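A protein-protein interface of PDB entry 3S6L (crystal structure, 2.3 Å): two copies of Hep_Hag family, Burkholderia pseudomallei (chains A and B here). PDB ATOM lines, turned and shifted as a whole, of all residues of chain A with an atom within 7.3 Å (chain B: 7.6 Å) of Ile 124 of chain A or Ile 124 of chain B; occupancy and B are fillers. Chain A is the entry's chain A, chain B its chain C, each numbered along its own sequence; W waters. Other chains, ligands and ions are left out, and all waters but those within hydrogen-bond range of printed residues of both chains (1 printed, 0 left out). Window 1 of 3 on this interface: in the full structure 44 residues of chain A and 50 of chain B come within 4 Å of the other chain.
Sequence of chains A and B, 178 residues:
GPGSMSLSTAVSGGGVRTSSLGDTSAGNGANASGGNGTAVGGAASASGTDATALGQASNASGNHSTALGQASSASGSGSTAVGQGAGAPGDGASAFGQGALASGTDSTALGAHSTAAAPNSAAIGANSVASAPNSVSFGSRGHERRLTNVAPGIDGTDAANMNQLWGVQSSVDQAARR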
ATOM      1  N   THR A 108      -9.410  25.594  19.708  1.00  0.00           N
ATOM      2  CA  THR A 108      -9.409  24.219  20.145  1.00  0.00           C
ATOM      3  C   THR A 108     -10.049  23.427  19.032  1.00  0.00           C
ATOM      4  O   THR A 108     -11.216  23.681  18.664  1.00  0.00           O
ATOM      5  CB  THR A 108     -10.213  24.057  21.479  1.00  0.00           C
ATOM      6  OG1 THR A 108      -9.695  24.968  22.458  1.00  0.00           O
ATOM      7  CG2 THR A 108     -10.125  22.638  22.018  1.00  0.00           C
ATOM      8  N   ALA A 109      -9.271  22.513  18.459  1.00  0.00           N
ATOM      9  CA  ALA A 109      -9.713  21.684  17.336  1.00  0.00           C
ATOM     10  C   ALA A 109      -9.730  20.239  17.767  1.00  0.00           C
ATOM     11  O   ALA A 109      -8.663  19.670  18.048  1.00  0.00           O
ATOM     12  CB  ALA A 109      -8.787  21.870  16.110  1.00  0.00           C
ATOM     13  N   LEU A 110     -10.927  19.643  17.793  1.00  0.00           N
ATOM     14  CA  LEU A 110     -11.135  18.284  18.316  1.00  0.00           C
ATOM     15  C   LEU A 110     -11.755  17.353  17.275  1.00  0.00           C
ATOM     16  O   LEU A 110     -12.971  17.372  17.050  1.00  0.00           O
ATOM     17  CB  LEU A 110     -12.019  18.371  19.573  1.00  0.00           C
ATOM     18  CG  LEU A 110     -11.451  19.258  20.697  1.00  0.00           C
ATOM     19  CD1 LEU A 110     -12.496  19.510  21.737  1.00  0.00           C
ATOM     20  CD2 LEU A 110     -10.236  18.649  21.344  1.00  0.00           C
ATOM     21  N   GLY A 111     -10.930  16.564  16.603  1.00  0.00           N
ATOM     22  CA  GLY A 111     -11.410  15.677  15.541  1.00  0.00           C
ATOM     23  C   GLY A 111     -10.494  15.714  14.323  1.00  0.00           C
ATOM     24  O   GLY A 111      -9.889  16.758  14.014  1.00  0.00           O
ATOM     25  N   SER A 114     -10.174  18.585  11.593  1.00  0.00           N
ATOM     26  CA  SER A 114     -10.947  19.735  12.059  1.00  0.00           C
ATOM     27  C   SER A 114     -10.015  20.946  12.043  1.00  0.00           C
ATOM     28  O   SER A 114      -8.807  20.789  12.193  1.00  0.00           O
ATOM     29  CB  SER A 114     -11.462  19.523  13.479  1.00  0.00           C
ATOM     30  OG  SER A 114     -10.351  19.316  14.369  1.00  0.00           O
ATOM     31  N   THR A 115     -10.579  22.137  11.869  1.00  0.00           N
ATOM     32  CA  THR A 115      -9.802  23.378  11.777  1.00  0.00           C
ATOM     33  C   THR A 115     -10.491  24.438  12.653  1.00  0.00           C
ATOM     34  O   THR A 115     -11.643  24.810  12.408  1.00  0.00           O
ATOM     35  CB  THR A 115      -9.678  23.908  10.292  1.00  0.00           C
ATOM     36  OG1 THR A 115      -9.093  22.896   9.444  1.00  0.00           O
ATOM     37  CG2 THR A 115      -8.813  25.216  10.205  1.00  0.00           C
ATOM     38  N   ALA A 116      -9.815  24.866  13.703  1.00  0.00           N
ATOM     39  CA  ALA A 116     -10.308  25.965  14.529  1.00  0.00           C
ATOM     40  C   ALA A 116      -9.436  27.156  14.203  1.00  0.00           C
ATOM     41  O   ALA A 116      -8.326  27.307  14.754  1.00  0.00           O
ATOM     42  CB  ALA A 116     -10.253  25.638  16.004  1.00  0.00           C
ATOM     43  N   ALA A 122     -13.835  27.040  18.622  1.00  0.00           N
ATOM     44  CA  ALA A 122     -13.645  25.612  18.710  1.00  0.00           C
ATOM     45  C   ALA A 122     -14.308  24.873  17.566  1.00  0.00           C
ATOM     46  O   ALA A 122     -15.411  25.223  17.127  1.00  0.00           O
ATOM     47  CB  ALA A 122     -14.157  25.059  20.076  1.00  0.00           C
ATOM     48  N   ALA A 123     -13.639  23.821  17.116  1.00  0.00           N
ATOM     49  CA  ALA A 123     -14.167  22.965  16.064  1.00  0.00           C
ATOM     50  C   ALA A 123     -14.273  21.581  16.653  1.00  0.00           C
ATOM     51  O   ALA A 123     -13.251  21.029  17.104  1.00  0.00           O
ATOM     52  CB  ALA A 123     -13.233  22.971  14.855  1.00  0.00           C
ATOM     53  N   ILE A 124     -15.494  21.039  16.675  1.00  0.00           N
ATOM     54  CA  ILE A 124     -15.776  19.713  17.254  1.00  0.00           C
ATOM     55  C   ILE A 124     -16.239  18.763  16.148  1.00  0.00           C
ATOM     56  O   ILE A 124     -17.236  19.028  15.459  1.00  0.00           O
ATOM     57  CB  ILE A 124     -16.919  19.790  18.310  1.00  0.00           C
ATOM     58  CG1 ILE A 124     -16.644  20.822  19.401  1.00  0.00           C
ATOM     59  CG2 ILE A 124     -17.189  18.455  18.946  1.00  0.00           C
ATOM     60  CD1 ILE A 124     -15.335  20.623  20.109  1.00  0.00           C
ATOM     61  N   GLY A 125     -15.529  17.653  15.976  1.00  0.00           N
ATOM     62  CA  GLY A 125     -15.965  16.636  15.034  1.00  0.00           C
ATOM     63  C   GLY A 125     -15.042  16.593  13.840  1.00  0.00           C
ATOM     64  O   GLY A 125     -14.425  17.598  13.504  1.00  0.00           O
ATOM     65  N   ALA A 126     -14.926  15.420  13.220  1.00  0.00           N
ATOM     66  CA  ALA A 126     -14.096  15.261  12.056  1.00  0.00           C
ATOM     67  C   ALA A 126     -14.487  16.290  10.951  1.00  0.00           C
ATOM     68  O   ALA A 126     -15.691  16.515  10.700  1.00  0.00           O
ATOM     69  CB  ALA A 126     -14.209  13.834  11.540  1.00  0.00           C
ATOM     70  N   ASN A 127     -13.482  16.921  10.326  1.00  0.00           N
ATOM     71  CA  ASN A 127     -13.706  17.874   9.219  1.00  0.00           C
ATOM     72  C   ASN A 127     -14.462  19.153   9.613  1.00  0.00           C
ATOM     73  O   ASN A 127     -14.814  19.954   8.736  1.00  0.00           O
ATOM     74  CB  ASN A 127     -14.446  17.177   8.050  1.00  0.00           C
ATOM     75  CG  ASN A 127     -13.715  15.920   7.556  1.00  0.00           C
ATOM     76  OD1 ASN A 127     -14.250  14.801   7.597  1.00  0.00           O
ATOM     77  ND2 ASN A 127     -12.490  16.097   7.115  1.00  0.00           N
ATOM     78  N   SER A 128     -14.739  19.341  10.905  1.00  0.00           N
ATOM     79  CA  SER A 128     -15.430  20.562  11.348  1.00  0.00           C
ATOM     80  C   SER A 128     -14.550  21.799  11.166  1.00  0.00           C
ATOM     81  O   SER A 128     -13.322  21.737  11.363  1.00  0.00           O
ATOM     82  CB  SER A 128     -15.868  20.473  12.825  1.00  0.00           C
ATOM     83  OG  SER A 128     -16.925  19.550  12.968  1.00  0.00           O
ATOM     84  N   VAL A 129     -15.179  22.924  10.819  1.00  0.00           N
ATOM     85  CA  VAL A 129     -14.446  24.175  10.619  1.00  0.00           C
ATOM     86  C   VAL A 129     -15.080  25.267  11.478  1.00  0.00           C
ATOM     87  O   VAL A 129     -16.318  25.401  11.514  1.00  0.00           O
ATOM     88  CB  VAL A 129     -14.441  24.590   9.149  1.00  0.00           C
ATOM     89  CG1 VAL A 129     -13.580  25.870   8.927  1.00  0.00           C
ATOM     90  CG2 VAL A 129     -13.939  23.455   8.268  1.00  0.00           C
ATOM     91  N   ALA A 130     -14.229  26.003  12.203  1.00  0.00           N
ATOM     92  CA  ALA A 130     -14.662  27.131  13.010  1.00  0.00           C
ATOM     93  C   ALA A 130     -13.984  28.385  12.497  1.00  0.00           C
ATOM     94  O   ALA A 130     -12.785  28.591  12.731  1.00  0.00           O
ATOM     95  CB  ALA A 130     -14.347  26.915  14.516  1.00  0.00           C
ATOM     96  N   VAL A 136     -18.401  27.959  18.579  1.00  0.00           N
ATOM     97  CA  VAL A 136     -18.047  26.540  18.610  1.00  0.00           C
ATOM     98  C   VAL A 136     -18.776  25.889  17.459  1.00  0.00           C
ATOM     99  O   VAL A 136     -20.000  25.898  17.449  1.00  0.00           O
ATOM    100  CB  VAL A 136     -18.469  25.887  19.934  1.00  0.00           C
ATOM    101  CG1 VAL A 136     -18.139  24.412  19.923  1.00  0.00           C
ATOM    102  CG2 VAL A 136     -17.789  26.575  21.092  1.00  0.00           C
ATOM    103  N   SER A 137     -18.038  25.347  16.486  1.00  0.00           N
ATOM    104  CA  SER A 137     -18.636  24.704  15.332  1.00  0.00           C
ATOM    105  C   SER A 137     -18.703  23.178  15.424  1.00  0.00           C
ATOM    106  O   SER A 137     -17.708  22.511  15.785  1.00  0.00           O
ATOM    107  CB  SER A 137     -17.870  25.091  14.068  1.00  0.00           C
ATOM    108  OG  SER A 137     -18.323  24.298  12.970  1.00  0.00           O
ATOM    109  N   PHE A 138     -19.847  22.617  15.017  1.00  0.00           N
ATOM    110  CA  PHE A 138     -20.008  21.169  14.990  1.00  0.00           C
ATOM    111  C   PHE A 138     -19.979  20.593  13.568  1.00  0.00           C
ATOM    112  O   PHE A 138     -20.416  19.470  13.332  1.00  0.00           O
ATOM    113  CB  PHE A 138     -21.284  20.750  15.757  1.00  0.00           C
ATOM    114  CG  PHE A 138     -21.261  21.149  17.196  1.00  0.00           C
ATOM    115  CD1 PHE A 138     -20.673  20.323  18.145  1.00  0.00           C
ATOM    116  CD2 PHE A 138     -21.786  22.381  17.604  1.00  0.00           C
ATOM    117  CE1 PHE A 138     -20.642  20.700  19.484  1.00  0.00           C
ATOM    118  CE2 PHE A 138     -21.746  22.771  18.948  1.00  0.00           C
ATOM    119  CZ  PHE A 138     -21.187  21.934  19.881  1.00  0.00           C
ATOM    120  N   GLY A 139     -19.443  21.352  12.625  1.00  0.00           N
ATOM    121  CA  GLY A 139     -19.403  20.889  11.246  1.00  0.00           C
ATOM    122  C   GLY A 139     -18.964  22.009  10.334  1.00  0.00           C
ATOM    123  O   GLY A 139     -17.969  22.686  10.599  1.00  0.00           O
ATOM    124  N   ARG A 145     -24.344  19.176  12.136  1.00  0.00           N
ATOM    125  CA  ARG A 145     -24.588  17.999  12.979  1.00  0.00           C
ATOM    126  C   ARG A 145     -25.646  18.322  13.991  1.00  0.00           C
ATOM    127  O   ARG A 145     -25.703  19.449  14.466  1.00  0.00           O
ATOM    128  CB  ARG A 145     -23.313  17.524  13.671  1.00  0.00           C
ATOM    129  CG  ARG A 145     -22.325  16.758  12.731  1.00  0.00           C
ATOM    130  CD  ARG A 145     -21.176  16.233  13.581  1.00  0.00           C
ATOM    131  NE  ARG A 145     -20.137  15.522  12.857  1.00  0.00           N
ATOM    132  CZ  ARG A 145     -19.007  16.087  12.445  1.00  0.00           C
ATOM    133  NH1 ARG A 145     -18.799  17.375  12.675  1.00  0.00           N
ATOM    134  NH2 ARG A 145     -18.081  15.370  11.798  1.00  0.00           N
ATOM    135  N   THR B 108     -15.576  10.769  16.721  1.00  0.00           N
ATOM    136  CA  THR B 108     -14.741  11.412  17.722  1.00  0.00           C
ATOM    137  C   THR B 108     -15.372  11.207  19.110  1.00  0.00           C
ATOM    138  O   THR B 108     -16.537  11.582  19.333  1.00  0.00           O
ATOM    139  CB  THR B 108     -14.602  12.921  17.383  1.00  0.00           C
ATOM    140  OG1 THR B 108     -14.213  13.056  15.999  1.00  0.00           O
ATOM    141  CG2 THR B 108     -13.569  13.608  18.252  1.00  0.00           C
ATOM    142  N   ALA B 109     -14.608  10.620  20.031  1.00  0.00           N
ATOM    143  CA  ALA B 109     -15.109  10.284  21.369  1.00  0.00           C
ATOM    144  C   ALA B 109     -14.231  10.958  22.392  1.00  0.00           C
ATOM    145  O   ALA B 109     -13.043  10.641  22.501  1.00  0.00           O
ATOM    146  CB  ALA B 109     -15.121   8.738  21.594  1.00  0.00           C
ATOM    147  N   LEU B 110     -14.794  11.907  23.128  1.00  0.00           N
ATOM    148  CA  LEU B 110     -13.996  12.764  24.013  1.00  0.00           C
ATOM    149  C   LEU B 110     -14.602  12.710  25.414  1.00  0.00           C
ATOM    150  O   LEU B 110     -15.644  13.330  25.685  1.00  0.00           O
ATOM    151  CB  LEU B 110     -13.947  14.195  23.462  1.00  0.00           C
ATOM    152  CG  LEU B 110     -13.594  14.415  21.964  1.00  0.00           C
ATOM    153  CD1 LEU B 110     -13.854  15.837  21.559  1.00  0.00           C
ATOM    154  CD2 LEU B 110     -12.142  14.112  21.661  1.00  0.00           C
ATOM    155  N   GLY B 111     -13.950  11.933  26.286  1.00  0.00           N
ATOM    156  CA  GLY B 111     -14.434  11.626  27.625  1.00  0.00           C
ATOM    157  C   GLY B 111     -14.220  10.161  28.002  1.00  0.00           C
ATOM    158  O   GLY B 111     -14.357   9.264  27.163  1.00  0.00           O
ATOM    159  N   SER B 114     -16.523   7.123  26.881  1.00  0.00           N
ATOM    160  CA  SER B 114     -17.454   7.641  25.876  1.00  0.00           C
ATOM    161  C   SER B 114     -17.384   6.701  24.677  1.00  0.00           C
ATOM    162  O   SER B 114     -16.378   6.001  24.493  1.00  0.00           O
ATOM    163  CB  SER B 114     -17.072   9.062  25.456  1.00  0.00           C
ATOM    164  OG  SER B 114     -15.782   9.068  24.856  1.00  0.00           O
ATOM    165  N   THR B 115     -18.439   6.681  23.863  1.00  0.00           N
ATOM    166  CA  THR B 115     -18.453   5.819  22.707  1.00  0.00           C
ATOM    167  C   THR B 115     -19.104   6.555  21.564  1.00  0.00           C
ATOM    168  O   THR B 115     -20.258   6.978  21.679  1.00  0.00           O
ATOM    169  CB  THR B 115     -19.277   4.517  22.951  1.00  0.00           C
ATOM    170  OG1 THR B 115     -18.764   3.802  24.081  1.00  0.00           O
ATOM    171  CG2 THR B 115     -19.226   3.614  21.715  1.00  0.00           C
ATOM    172  N   ALA B 116     -18.378   6.710  20.460  1.00  0.00           N
ATOM    173  CA  ALA B 116     -18.966   7.209  19.232  1.00  0.00           C
ATOM    174  C   ALA B 116     -18.911   6.097  18.180  1.00  0.00           C
ATOM    175  O   ALA B 116     -17.891   5.899  17.491  1.00  0.00           O
ATOM    176  CB  ALA B 116     -18.236   8.459  18.752  1.00  0.00           C
ATOM    177  N   ALA B 122     -20.014  12.334  17.164  1.00  0.00           N
ATOM    178  CA  ALA B 122     -19.160  12.720  18.258  1.00  0.00           C
ATOM    179  C   ALA B 122     -19.862  12.474  19.571  1.00  0.00           C
ATOM    180  O   ALA B 122     -21.052  12.729  19.693  1.00  0.00           O
ATOM    181  CB  ALA B 122     -18.733  14.178  18.119  1.00  0.00           C
ATOM    182  N   ALA B 123     -19.113  11.974  20.551  1.00  0.00           N
ATOM    183  CA  ALA B 123     -19.604  11.806  21.911  1.00  0.00           C
ATOM    184  C   ALA B 123     -18.747  12.684  22.829  1.00  0.00           C
ATOM    185  O   ALA B 123     -17.492  12.591  22.818  1.00  0.00           O
ATOM    186  CB  ALA B 123     -19.560  10.334  22.315  1.00  0.00           C
ATOM    187  N   ILE B 124     -19.418  13.569  23.584  1.00  0.00           N
ATOM    188  CA  ILE B 124     -18.734  14.553  24.408  1.00  0.00           C
ATOM    189  C   ILE B 124     -19.136  14.282  25.831  1.00  0.00           C
ATOM    190  O   ILE B 124     -20.329  14.335  26.166  1.00  0.00           O
ATOM    191  CB  ILE B 124     -19.168  16.017  24.097  1.00  0.00           C
ATOM    192  CG1 ILE B 124     -19.027  16.391  22.609  1.00  0.00           C
ATOM    193  CG2 ILE B 124     -18.467  17.017  25.046  1.00  0.00           C
ATOM    194  CD1 ILE B 124     -17.575  16.497  22.118  1.00  0.00           C
ATOM    195  N   GLY B 125     -18.138  14.035  26.679  1.00  0.00           N
ATOM    196  CA  GLY B 125     -18.378  13.828  28.115  1.00  0.00           C
ATOM    197  C   GLY B 125     -18.246  12.351  28.479  1.00  0.00           C
ATOM    198  O   GLY B 125     -18.428  11.496  27.618  1.00  0.00           O
ATOM    199  N   ALA B 126     -17.902  12.071  29.743  1.00  0.00           N
ATOM    200  CA  ALA B 126     -17.754  10.714  30.243  1.00  0.00           C
ATOM    201  C   ALA B 126     -19.043   9.929  29.994  1.00  0.00           C
ATOM    202  O   ALA B 126     -20.142  10.438  30.244  1.00  0.00           O
ATOM    203  CB  ALA B 126     -17.425  10.720  31.754  1.00  0.00           C
ATOM    204  N   ASN B 127     -18.884   8.695  29.511  1.00  0.00           N
ATOM    205  CA  ASN B 127     -19.987   7.751  29.294  1.00  0.00           C
ATOM    206  C   ASN B 127     -20.966   8.187  28.231  1.00  0.00           C
ATOM    207  O   ASN B 127     -21.968   7.525  28.049  1.00  0.00           O
ATOM    208  CB  ASN B 127     -20.739   7.441  30.603  1.00  0.00           C
ATOM    209  CG  ASN B 127     -19.791   6.903  31.713  1.00  0.00           C
ATOM    210  OD1 ASN B 127     -19.604   7.536  32.750  1.00  0.00           O
ATOM    211  ND2 ASN B 127     -19.212   5.743  31.486  1.00  0.00           N
ATOM    212  N   SER B 128     -20.697   9.285  27.524  1.00  0.00           N
ATOM    213  CA  SER B 128     -21.588   9.683  26.433  1.00  0.00           C
ATOM    214  C   SER B 128     -21.595   8.655  25.306  1.00  0.00           C
ATOM    215  O   SER B 128     -20.578   8.036  25.028  1.00  0.00           O
ATOM    216  CB  SER B 128     -21.236  11.061  25.886  1.00  0.00           C
ATOM    217  OG  SER B 128     -21.370  12.003  26.934  1.00  0.00           O
ATOM    218  N   VAL B 129     -22.752   8.495  24.662  1.00  0.00           N
ATOM    219  CA  VAL B 129     -22.915   7.536  23.582  1.00  0.00           C
ATOM    220  C   VAL B 129     -23.418   8.264  22.352  1.00  0.00           C
ATOM    221  O   VAL B 129     -24.488   8.870  22.379  1.00  0.00           O
ATOM    222  CB  VAL B 129     -23.936   6.431  23.978  1.00  0.00           C
ATOM    223  CG1 VAL B 129     -24.256   5.480  22.777  1.00  0.00           C
ATOM    224  CG2 VAL B 129     -23.457   5.649  25.257  1.00  0.00           C
ATOM    225  N   ALA B 130     -22.661   8.217  21.262  1.00  0.00           N
ATOM    226  CA  ALA B 130     -23.202   8.728  19.987  1.00  0.00           C
ATOM    227  C   ALA B 130     -23.537   7.546  19.077  1.00  0.00           C
ATOM    228  O   ALA B 130     -22.625   6.900  18.552  1.00  0.00           O
ATOM    229  CB  ALA B 130     -22.222   9.729  19.292  1.00  0.00           C
ATOM    230  N   VAL B 136     -23.816  14.928  17.373  1.00  0.00           N
ATOM    231  CA  VAL B 136     -22.920  15.108  18.521  1.00  0.00           C
ATOM    232  C   VAL B 136     -23.764  14.868  19.765  1.00  0.00           C
ATOM    233  O   VAL B 136     -24.724  15.618  20.002  1.00  0.00           O
ATOM    234  CB  VAL B 136     -22.351  16.540  18.575  1.00  0.00           C
ATOM    235  CG1 VAL B 136     -21.340  16.695  19.732  1.00  0.00           C
ATOM    236  CG2 VAL B 136     -21.700  16.922  17.236  1.00  0.00           C
ATOM    237  N   SER B 137     -23.427  13.827  20.533  1.00  0.00           N
ATOM    238  CA  SER B 137     -24.124  13.491  21.810  1.00  0.00           C
ATOM    239  C   SER B 137     -23.376  14.002  23.041  1.00  0.00           C
ATOM    240  O   SER B 137     -22.132  13.909  23.131  1.00  0.00           O
ATOM    241  CB  SER B 137     -24.322  11.970  21.931  1.00  0.00           C
ATOM    242  OG  SER B 137     -24.915  11.565  23.168  1.00  0.00           O
ATOM    243  N   PHE B 138     -24.130  14.532  23.990  1.00  0.00           N
ATOM    244  CA  PHE B 138     -23.572  15.032  25.249  1.00  0.00           C
ATOM    245  C   PHE B 138     -23.998  14.149  26.406  1.00  0.00           C
ATOM    246  O   PHE B 138     -23.854  14.522  27.557  1.00  0.00           O
ATOM    247  CB  PHE B 138     -24.003  16.476  25.479  1.00  0.00           C
ATOM    248  CG  PHE B 138     -23.565  17.386  24.393  1.00  0.00           C
ATOM    249  CD1 PHE B 138     -22.366  18.057  24.482  1.00  0.00           C
ATOM    250  CD2 PHE B 138     -24.334  17.558  23.255  1.00  0.00           C
ATOM    251  CE1 PHE B 138     -21.950  18.892  23.469  1.00  0.00           C
ATOM    252  CE2 PHE B 138     -23.899  18.401  22.237  1.00  0.00           C
ATOM    253  CZ  PHE B 138     -22.706  19.053  22.355  1.00  0.00           C
ATOM    254  N   GLY B 139     -24.512  12.966  26.091  1.00  0.00           N
ATOM    255  CA  GLY B 139     -24.788  11.969  27.117  1.00  0.00           C
ATOM    256  C   GLY B 139     -25.387  10.726  26.488  1.00  0.00           C
ATOM    257  O   GLY B 139     -24.830  10.181  25.547  1.00  0.00           O
ATOM    258  N   SER B 140     -26.513  10.280  27.036  1.00  0.00           N
ATOM    259  CA  SER B 140     -27.254   9.128  26.549  1.00  0.00           C
ATOM    260  C   SER B 140     -28.645   9.285  27.162  1.00  0.00           C
ATOM    261  O   SER B 140     -28.833  10.143  28.051  1.00  0.00           O
ATOM    262  CB  SER B 140     -26.607   7.828  27.032  1.00  0.00           C
ATOM    263  OG  SER B 140     -26.575   7.796  28.454  1.00  0.00           O
ATOM    264  N   ARG B 145     -27.280  15.965  29.360  1.00  0.00           N
ATOM    265  CA  ARG B 145     -26.523  17.037  29.985  1.00  0.00           C
ATOM    266  C   ARG B 145     -27.023  18.344  29.428  1.00  0.00           C
ATOM    267  O   ARG B 145     -27.428  18.417  28.274  1.00  0.00           O
ATOM    268  CB  ARG B 145     -25.030  16.898  29.681  1.00  0.00           C
ATOM    269  CG  ARG B 145     -24.281  15.935  30.596  1.00  0.00           C
ATOM    270  CD  ARG B 145     -22.766  15.977  30.313  1.00  0.00           C
ATOM    271  NE  ARG B 145     -22.042  14.963  31.076  1.00  0.00           N
ATOM    272  CZ  ARG B 145     -21.698  13.763  30.606  1.00  0.00           C
ATOM    273  NH1 ARG B 145     -22.005  13.402  29.343  1.00  0.00           N
ATOM    274  NH2 ARG B 145     -21.034  12.927  31.395  1.00  0.00           N
ATOM    275  N   LEU B 147     -26.561  22.330  28.253  1.00  0.00           N
ATOM    276  CA  LEU B 147     -25.503  23.096  27.571  1.00  0.00           C
ATOM    277  C   LEU B 147     -25.520  24.536  28.057  1.00  0.00           C
ATOM    278  O   LEU B 147     -26.573  25.194  28.004  1.00  0.00           O
ATOM    279  CB  LEU B 147     -25.634  23.055  26.036  1.00  0.00           C
ATOM    280  CG  LEU B 147     -25.838  21.708  25.323  1.00  0.00           C
ATOM    281  CD1 LEU B 147     -25.791  21.837  23.802  1.00  0.00           C
ATOM    282  CD2 LEU B 147     -24.809  20.697  25.774  1.00  0.00           C
HETATM  283  O   HOH W   1     -16.382  13.063  14.473  1.00  0.00           O
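Leu 110 of chain A touches its own counterpart, Leu 110 of chain B.
Gly 111 of chain A touches Thr 108 of chain B, but with the chains exchanged Thr 108 of chain A does not touch Gly 111 of chain B (12.1 Å).
Ile 124 of chain A touches its own counterpart, Ile 124 of chain B.
Arg 145 of chain A touches Val 136 of chain B, but with the chains exchanged Val 136 of chain A does not touch Arg 145 of chain B (13.9 Å).
21 positions are printed for both chains.
Water W1 bridges OG1 of Thr 108 of chain B (2.7 Å) and N of Ala 126 of chain A (3.0 Å).
Among the printed residues, merely in contact across the chains: Leu 110 of chain A with Thr 108 of chain B, Leu 110 of chain A with Leu 110 of chain B, Gly 111 of chain A with Thr 108 of chain B, Ile 124 of chain A with Ile 124 of chain B, Ala 126 of chain A with Thr 108 of chain B, Phe 138 of chain A with Val 136 of chain B, Phe 138 of chain A with Phe 138 of chain B and Arg 145 of chain A with Val 136 of chain B.
The backbone carbonyl oxygen (O) of Leu 110 of chain A is in hydrogen-bond range of the backbone NH (N) of Gly 125 of chain A, 2.8 Å away.
The backbone NH of Leu 110 of chain B sits at hydrogen-bond distance from the backbone carbonyl oxygen of Ala 123 of chain B, at 2.8 Å.
The backbone NH (N) of Leu 110 of chain A sits at hydrogen-bond distance from the backbone carbonyl oxygen (O) of Ala 123 of chain A.
N of Ile 124 of chain B sits at hydrogen-bond distance from O of Ser 137 of chain B (2.8 Å).
The backbone carbonyl oxygen (O) of Thr 108 of chain B sits at hydrogen-bond distance from the backbone NH (N) of Ala 123 of chain B (2.9 Å).
NH1 of Arg 145 of chain A sits at hydrogen-bond distance from O of Phe 138 of chain A, at 2.7 Å.
Of the 21 printed residues of chain A, 6 touch a printed residue of chain B.
Printed residues of chain A that touch a printed residue of chain B: Leu 110, Gly 111, Ile 124, Ala 126, Phe 138 and Arg 145.
Hydrophobic or aromatic side chains of chain A within 4 Å of the printed part of chain B: Leu 110, Ile 124 and Phe 138.
Among the printed residues, no Asp or Glu carboxylate lies within 4 Å of a Lys or Arg side-chain nitrogen of the other chain.
Of chain B, only Ile 124 (3.7 Å) comes within 4 Å of Ile 124 of chain A.
No residue of chain B comes within 4 Å of Ala 123 of chain A.
Gly 125 of chain A touches none of the printed residues of chain B.
Of the printed residues of chain B, Leu 110 of chain A touches Thr 108 and Leu 110.
Of the printed residues of chain A, Thr 108 of chain B touches Leu 110 (3.996 Å), Gly 111 (3.9 Å) and Ala 126 (3.7 Å).
Gly 125 of chain B touches none of the printed residues of chain A.
The nearest residue of chain B that does not touch Ile 124 of chain A is Val 136 of chain B (4.6 Å).
The nearest residue of chain A that does not touch Ile 124 of chain B is Phe 138 of chain A (5.6 Å).
The nearest printed residue of chain B that does not touch Phe 138 of chain A is Ile 124 of chain B (5.6 Å).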
